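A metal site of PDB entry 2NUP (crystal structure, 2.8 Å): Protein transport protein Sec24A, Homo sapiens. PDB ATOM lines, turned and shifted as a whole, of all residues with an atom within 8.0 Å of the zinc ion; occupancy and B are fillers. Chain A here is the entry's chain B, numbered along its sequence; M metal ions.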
ATOM      1  N   ARG A  90     -12.787 -16.611 -11.138  1.00  0.00           N
ATOM      2  CA  ARG A  90     -13.552 -15.363 -11.157  1.00  0.00           C
ATOM      3  C   ARG A  90     -13.026 -14.363 -10.140  1.00  0.00           C
ATOM      4  O   ARG A  90     -13.107 -14.607  -8.941  1.00  0.00           O
ATOM      5  CB  ARG A  90     -15.019 -15.616 -10.809  1.00  0.00           C
ATOM      6  CG  ARG A  90     -15.717 -16.621 -11.687  1.00  0.00           C
ATOM      7  CD  ARG A  90     -17.166 -16.756 -11.268  1.00  0.00           C
ATOM      8  NE  ARG A  90     -17.904 -15.502 -11.399  1.00  0.00           N
ATOM      9  CZ  ARG A  90     -19.202 -15.373 -11.161  1.00  0.00           C
ATOM     10  NH1 ARG A  90     -19.905 -16.424 -10.776  1.00  0.00           N
ATOM     11  NH2 ARG A  90     -19.803 -14.201 -11.314  1.00  0.00           N
ATOM     12  N   CYS A  91     -12.507 -13.223 -10.608  1.00  0.00           N
ATOM     13  CA  CYS A  91     -12.003 -12.194  -9.711  1.00  0.00           C
ATOM     14  C   CYS A  91     -12.747 -12.229  -8.373  1.00  0.00           C
ATOM     15  O   CYS A  91     -13.982 -12.302  -8.351  1.00  0.00           O
ATOM     16  CB  CYS A  91     -12.167 -10.819 -10.346  1.00  0.00           C
ATOM     17  SG  CYS A  91     -12.315  -9.513  -9.118  1.00  0.00           S
ATOM     18  N   ARG A  92     -11.997 -12.179  -7.282  1.00  0.00           N
ATOM     19  CA  ARG A  92     -12.582 -12.226  -5.938  1.00  0.00           C
ATOM     20  C   ARG A  92     -13.388 -11.000  -5.554  1.00  0.00           C
ATOM     21  O   ARG A  92     -14.173 -11.042  -4.609  1.00  0.00           O
ATOM     22  CB  ARG A  92     -11.483 -12.428  -4.891  1.00  0.00           C
ATOM     23  CG  ARG A  92     -10.731 -13.739  -4.990  1.00  0.00           C
ATOM     24  CD  ARG A  92      -9.763 -13.849  -3.829  1.00  0.00           C
ATOM     25  NE  ARG A  92      -9.043 -15.133  -3.831  1.00  0.00           N
ATOM     26  CZ  ARG A  92      -8.178 -15.489  -2.894  1.00  0.00           C
ATOM     27  NH1 ARG A  92      -7.921 -14.679  -1.871  1.00  0.00           N
ATOM     28  NH2 ARG A  92      -7.564 -16.667  -2.974  1.00  0.00           N
ATOM     29  N   SER A  93     -13.195  -9.906  -6.265  1.00  0.00           N
ATOM     30  CA  SER A  93     -13.909  -8.683  -5.959  1.00  0.00           C
ATOM     31  C   SER A  93     -15.225  -8.566  -6.710  1.00  0.00           C
ATOM     32  O   SER A  93     -16.292  -8.740  -6.127  1.00  0.00           O
ATOM     33  CB  SER A  93     -13.047  -7.449  -6.259  1.00  0.00           C
ATOM     34  OG  SER A  93     -12.020  -7.278  -5.289  1.00  0.00           O
ATOM     35  N   CYS A  94     -15.134  -8.291  -8.009  1.00  0.00           N
ATOM     36  CA  CYS A  94     -16.323  -8.097  -8.838  1.00  0.00           C
ATOM     37  C   CYS A  94     -16.890  -9.358  -9.500  1.00  0.00           C
ATOM     38  O   CYS A  94     -17.844  -9.277 -10.273  1.00  0.00           O
ATOM     39  CB  CYS A  94     -15.994  -7.084  -9.923  1.00  0.00           C
ATOM     40  SG  CYS A  94     -14.909  -7.767 -11.165  1.00  0.00           S
ATOM     41  N   ARG A  95     -16.309 -10.518  -9.210  1.00  0.00           N
ATOM     42  CA  ARG A  95     -16.768 -11.797  -9.747  1.00  0.00           C
ATOM     43  C   ARG A  95     -16.664 -11.977 -11.258  1.00  0.00           C
ATOM     44  O   ARG A  95     -17.293 -12.858 -11.831  1.00  0.00           O
ATOM     45  CB  ARG A  95     -18.206 -12.075  -9.310  1.00  0.00           C
ATOM     46  CG  ARG A  95     -18.410 -12.167  -7.795  1.00  0.00           C
ATOM     47  CD  ARG A  95     -17.247 -12.893  -7.104  1.00  0.00           C
ATOM     48  NE  ARG A  95     -16.961 -14.203  -7.679  1.00  0.00           N
ATOM     49  CZ  ARG A  95     -17.572 -15.337  -7.339  1.00  0.00           C
ATOM     50  NH1 ARG A  95     -18.528 -15.327  -6.414  1.00  0.00           N
ATOM     51  NH2 ARG A  95     -17.253 -16.475  -7.940  1.00  0.00           N
ATOM     52  N   THR A  96     -15.842 -11.152 -11.910  1.00  0.00           N
ATOM     53  CA  THR A  96     -15.645 -11.249 -13.356  1.00  0.00           C
ATOM     54  C   THR A  96     -14.902 -12.529 -13.778  1.00  0.00           C
ATOM     55  O   THR A  96     -13.939 -12.940 -13.146  1.00  0.00           O
ATOM     56  CB  THR A  96     -14.875 -10.014 -13.872  1.00  0.00           C
ATOM     57  OG1 THR A  96     -15.688  -8.860 -13.696  1.00  0.00           O
ATOM     58  CG2 THR A  96     -14.506 -10.163 -15.335  1.00  0.00           C
ATOM     59  N   TYR A  97     -15.349 -13.145 -14.865  1.00  0.00           N
ATOM     60  CA  TYR A  97     -14.702 -14.347 -15.344  1.00  0.00           C
ATOM     61  C   TYR A  97     -13.337 -14.078 -15.988  1.00  0.00           C
ATOM     62  O   TYR A  97     -13.202 -13.224 -16.870  1.00  0.00           O
ATOM     63  CB  TYR A  97     -15.628 -15.052 -16.348  1.00  0.00           C
ATOM     64  CG  TYR A  97     -16.891 -15.588 -15.721  1.00  0.00           C
ATOM     65  CD1 TYR A  97     -16.909 -16.837 -15.120  1.00  0.00           C
ATOM     66  CD2 TYR A  97     -18.062 -14.828 -15.696  1.00  0.00           C
ATOM     67  CE1 TYR A  97     -18.060 -17.321 -14.505  1.00  0.00           C
ATOM     68  CE2 TYR A  97     -19.225 -15.307 -15.093  1.00  0.00           C
ATOM     69  CZ  TYR A  97     -19.220 -16.557 -14.499  1.00  0.00           C
ATOM     70  OH  TYR A  97     -20.348 -17.042 -13.891  1.00  0.00           O
ATOM     71  N   TRP A 110      -3.131 -12.367 -11.341  1.00  0.00           N
ATOM     72  CA  TRP A 110      -3.664 -11.675 -12.515  1.00  0.00           C
ATOM     73  C   TRP A 110      -4.525 -10.487 -12.084  1.00  0.00           C
ATOM     74  O   TRP A 110      -5.305 -10.574 -11.132  1.00  0.00           O
ATOM     75  CB  TRP A 110      -4.521 -12.627 -13.373  1.00  0.00           C
ATOM     76  CG  TRP A 110      -5.720 -13.228 -12.651  1.00  0.00           C
ATOM     77  CD1 TRP A 110      -5.732 -14.310 -11.816  1.00  0.00           C
ATOM     78  CD2 TRP A 110      -7.088 -12.779 -12.732  1.00  0.00           C
ATOM     79  NE1 TRP A 110      -7.003 -14.572 -11.377  1.00  0.00           N
ATOM     80  CE2 TRP A 110      -7.853 -13.648 -11.924  1.00  0.00           C
ATOM     81  CE3 TRP A 110      -7.725 -11.729 -13.413  1.00  0.00           C
ATOM     82  CZ2 TRP A 110      -9.245 -13.495 -11.778  1.00  0.00           C
ATOM     83  CZ3 TRP A 110      -9.097 -11.587 -13.257  1.00  0.00           C
ATOM     84  CH2 TRP A 110      -9.841 -12.462 -12.449  1.00  0.00           C
ATOM     85  N   LYS A 111      -4.383  -9.375 -12.796  1.00  0.00           N
ATOM     86  CA  LYS A 111      -5.138  -8.170 -12.499  1.00  0.00           C
ATOM     87  C   LYS A 111      -6.467  -8.152 -13.257  1.00  0.00           C
ATOM     88  O   LYS A 111      -6.476  -8.220 -14.490  1.00  0.00           O
ATOM     89  CB  LYS A 111      -4.316  -6.929 -12.876  1.00  0.00           C
ATOM     90  CG  LYS A 111      -5.087  -5.623 -12.786  1.00  0.00           C
ATOM     91  CD  LYS A 111      -4.201  -4.428 -13.032  1.00  0.00           C
ATOM     92  CE  LYS A 111      -3.219  -4.225 -11.882  1.00  0.00           C
ATOM     93  NZ  LYS A 111      -2.327  -3.051 -12.091  1.00  0.00           N
ATOM     94  N   CYS A 112      -7.576  -8.046 -12.513  1.00  0.00           N
ATOM     95  CA  CYS A 112      -8.924  -7.991 -13.105  1.00  0.00           C
ATOM     96  C   CYS A 112      -9.063  -6.786 -14.041  1.00  0.00           C
ATOM     97  O   CYS A 112      -8.780  -5.646 -13.637  1.00  0.00           O
ATOM     98  CB  CYS A 112      -9.986  -7.915 -11.989  1.00  0.00           C
ATOM     99  SG  CYS A 112     -11.688  -7.605 -12.571  1.00  0.00           S
ATOM    100  N   ASN A 113      -9.509  -7.016 -15.264  1.00  0.00           N
ATOM    101  CA  ASN A 113      -9.640  -5.903 -16.199  1.00  0.00           C
ATOM    102  C   ASN A 113     -10.931  -5.091 -16.046  1.00  0.00           C
ATOM    103  O   ASN A 113     -11.192  -4.167 -16.831  1.00  0.00           O
ATOM    104  CB  ASN A 113      -9.468  -6.404 -17.648  1.00  0.00           C
ATOM    105  CG  ASN A 113     -10.550  -7.354 -18.094  1.00  0.00           C
ATOM    106  OD1 ASN A 113     -10.978  -8.244 -17.354  1.00  0.00           O
ATOM    107  ND2 ASN A 113     -11.006  -7.185 -19.325  1.00  0.00           N
ATOM    108  N   LEU A 114     -11.725  -5.389 -15.028  1.00  0.00           N
ATOM    109  CA  LEU A 114     -12.946  -4.626 -14.805  1.00  0.00           C
ATOM    110  C   LEU A 114     -12.959  -3.854 -13.480  1.00  0.00           C
ATOM    111  O   LEU A 114     -13.577  -2.791 -13.379  1.00  0.00           O
ATOM    112  CB  LEU A 114     -14.169  -5.537 -14.916  1.00  0.00           C
ATOM    113  CG  LEU A 114     -14.719  -5.701 -16.341  1.00  0.00           C
ATOM    114  CD1 LEU A 114     -13.648  -6.254 -17.267  1.00  0.00           C
ATOM    115  CD2 LEU A 114     -15.921  -6.617 -16.304  1.00  0.00           C
ATOM    116  N   CYS A 115     -12.272  -4.374 -12.462  1.00  0.00           N
ATOM    117  CA  CYS A 115     -12.219  -3.707 -11.166  1.00  0.00           C
ATOM    118  C   CYS A 115     -10.783  -3.673 -10.641  1.00  0.00           C
ATOM    119  O   CYS A 115     -10.546  -3.422  -9.454  1.00  0.00           O
ATOM    120  CB  CYS A 115     -13.156  -4.376 -10.171  1.00  0.00           C
ATOM    121  SG  CYS A 115     -12.412  -5.546  -9.066  1.00  0.00           S
ATOM    122  N   TYR A 116      -9.837  -3.907 -11.546  1.00  0.00           N
ATOM    123  CA  TYR A 116      -8.399  -3.879 -11.294  1.00  0.00           C
ATOM    124  C   TYR A 116      -7.828  -4.616 -10.092  1.00  0.00           C
ATOM    125  O   TYR A 116      -6.622  -4.495  -9.821  1.00  0.00           O
ATOM    126  CB  TYR A 116      -7.897  -2.432 -11.233  1.00  0.00           C
ATOM    127  CG  TYR A 116      -8.521  -1.520 -12.259  1.00  0.00           C
ATOM    128  CD1 TYR A 116      -8.460  -1.808 -13.619  1.00  0.00           C
ATOM    129  CD2 TYR A 116      -9.178  -0.356 -11.857  1.00  0.00           C
ATOM    130  CE1 TYR A 116      -9.030  -0.955 -14.562  1.00  0.00           C
ATOM    131  CE2 TYR A 116      -9.750   0.492 -12.791  1.00  0.00           C
ATOM    132  CZ  TYR A 116      -9.673   0.198 -14.126  1.00  0.00           C
ATOM    133  OH  TYR A 116     -10.230   1.076 -15.037  1.00  0.00           O
ATOM    134  N   ARG A 117      -8.644  -5.361  -9.349  1.00  0.00           N
ATOM    135  CA  ARG A 117      -8.083  -6.102  -8.225  1.00  0.00           C
ATOM    136  C   ARG A 117      -7.201  -7.203  -8.777  1.00  0.00           C
ATOM    137  O   ARG A 117      -7.453  -7.733  -9.858  1.00  0.00           O
ATOM    138  CB  ARG A 117      -9.158  -6.735  -7.324  1.00  0.00           C
ATOM    139  CG  ARG A 117      -8.580  -7.881  -6.488  1.00  0.00           C
ATOM    140  CD  ARG A 117      -9.344  -8.197  -5.205  1.00  0.00           C
ATOM    141  NE  ARG A 117      -8.796  -9.399  -4.572  1.00  0.00           N
ATOM    142  CZ  ARG A 117      -9.187  -9.894  -3.404  1.00  0.00           C
ATOM    143  NH1 ARG A 117     -10.145  -9.299  -2.704  1.00  0.00           N
ATOM    144  NH2 ARG A 117      -8.633 -11.012  -2.946  1.00  0.00           N
ATOM    145  N   VAL A 118      -6.167  -7.545  -8.022  1.00  0.00           N
ATOM    146  CA  VAL A 118      -5.241  -8.598  -8.397  1.00  0.00           C
ATOM    147  C   VAL A 118      -5.713  -9.903  -7.758  1.00  0.00           C
ATOM    148  O   VAL A 118      -6.053  -9.923  -6.582  1.00  0.00           O
ATOM    149  CB  VAL A 118      -3.822  -8.288  -7.901  1.00  0.00           C
ATOM    150  CG1 VAL A 118      -2.837  -9.303  -8.457  1.00  0.00           C
ATOM    151  CG2 VAL A 118      -3.446  -6.885  -8.303  1.00  0.00           C
ATOM    152  N   ASN A 119      -5.726 -10.980  -8.544  1.00  0.00           N
ATOM    153  CA  ASN A 119      -6.163 -12.274  -8.048  1.00  0.00           C
ATOM    154  C   ASN A 119      -5.086 -13.348  -8.120  1.00  0.00           C
ATOM    155  O   ASN A 119      -4.208 -13.309  -8.996  1.00  0.00           O
ATOM    156  CB  ASN A 119      -7.400 -12.730  -8.804  1.00  0.00           C
ATOM    157  CG  ASN A 119      -8.663 -12.064  -8.313  1.00  0.00           C
ATOM    158  OD1 ASN A 119      -9.243 -12.467  -7.301  1.00  0.00           O
ATOM    159  ND2 ASN A 119      -9.102 -11.027  -9.029  1.00  0.00           N
ATOM    160  N   ARG A 412     -21.429  -6.941 -17.079  1.00  0.00           N
ATOM    161  CA  ARG A 412     -20.443  -6.183 -16.294  1.00  0.00           C
ATOM    162  C   ARG A 412     -19.638  -5.278 -17.203  1.00  0.00           C
ATOM    163  O   ARG A 412     -19.550  -5.531 -18.411  1.00  0.00           O
ATOM    164  CB  ARG A 412     -19.496  -7.139 -15.574  1.00  0.00           C
ATOM    165  CG  ARG A 412     -20.098  -7.982 -14.455  1.00  0.00           C
ATOM    166  CD  ARG A 412     -19.037  -8.879 -13.814  1.00  0.00           C
ATOM    167  NE  ARG A 412     -19.569  -9.647 -12.689  1.00  0.00           N
ATOM    168  CZ  ARG A 412     -20.386 -10.692 -12.817  1.00  0.00           C
ATOM    169  NH1 ARG A 412     -20.772 -11.105 -14.012  1.00  0.00           N
ATOM    170  NH2 ARG A 412     -20.858 -11.300 -11.730  1.00  0.00           N
HETATM  171 ZN    ZN M   1     -12.623  -7.542 -10.372  1.00  0.00          ZN
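The backbone NH (N) of Leu 114 sits close to the side-chain sulfur (SG) of Cys 112 (3.3 Å). SG of Cys 91 sits close to ND2 of Asn 119, 3.6 Å away. The side-chain sulfur of Cys 91 sits close to the backbone NH of Ser 93. The side-chain sulfur (SG) of Cys 94 sits close to the side-chain hydroxyl (OG1) of Thr 96 (2.9 Å). The backbone NH of Cys 112 sits at hydrogen-bond distance from the backbone carbonyl oxygen of Arg 117 (2.7 Å). The backbone NH (N) of Arg 117 sits close to the side-chain sulfur (SG) of Cys 115 (3.8 Å). O of Cys 94 sits at hydrogen-bond distance from NE of Arg 412 (3.0 Å). The backbone NH of Cys 91 is in hydrogen-bond range of the backbone carbonyl oxygen of Thr 96 (2.9 Å).
The zinc ion is bound by SG of Cys 91 (2.4 Å), SG of Cys 112 (2.4 Å), SG of Cys 115 (2.4 Å) and SG of Cys 94 (2.4 Å).
Within 4 Å of the zinc ion: Cys 91, Cys 94, Cys 112 and Cys 115.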
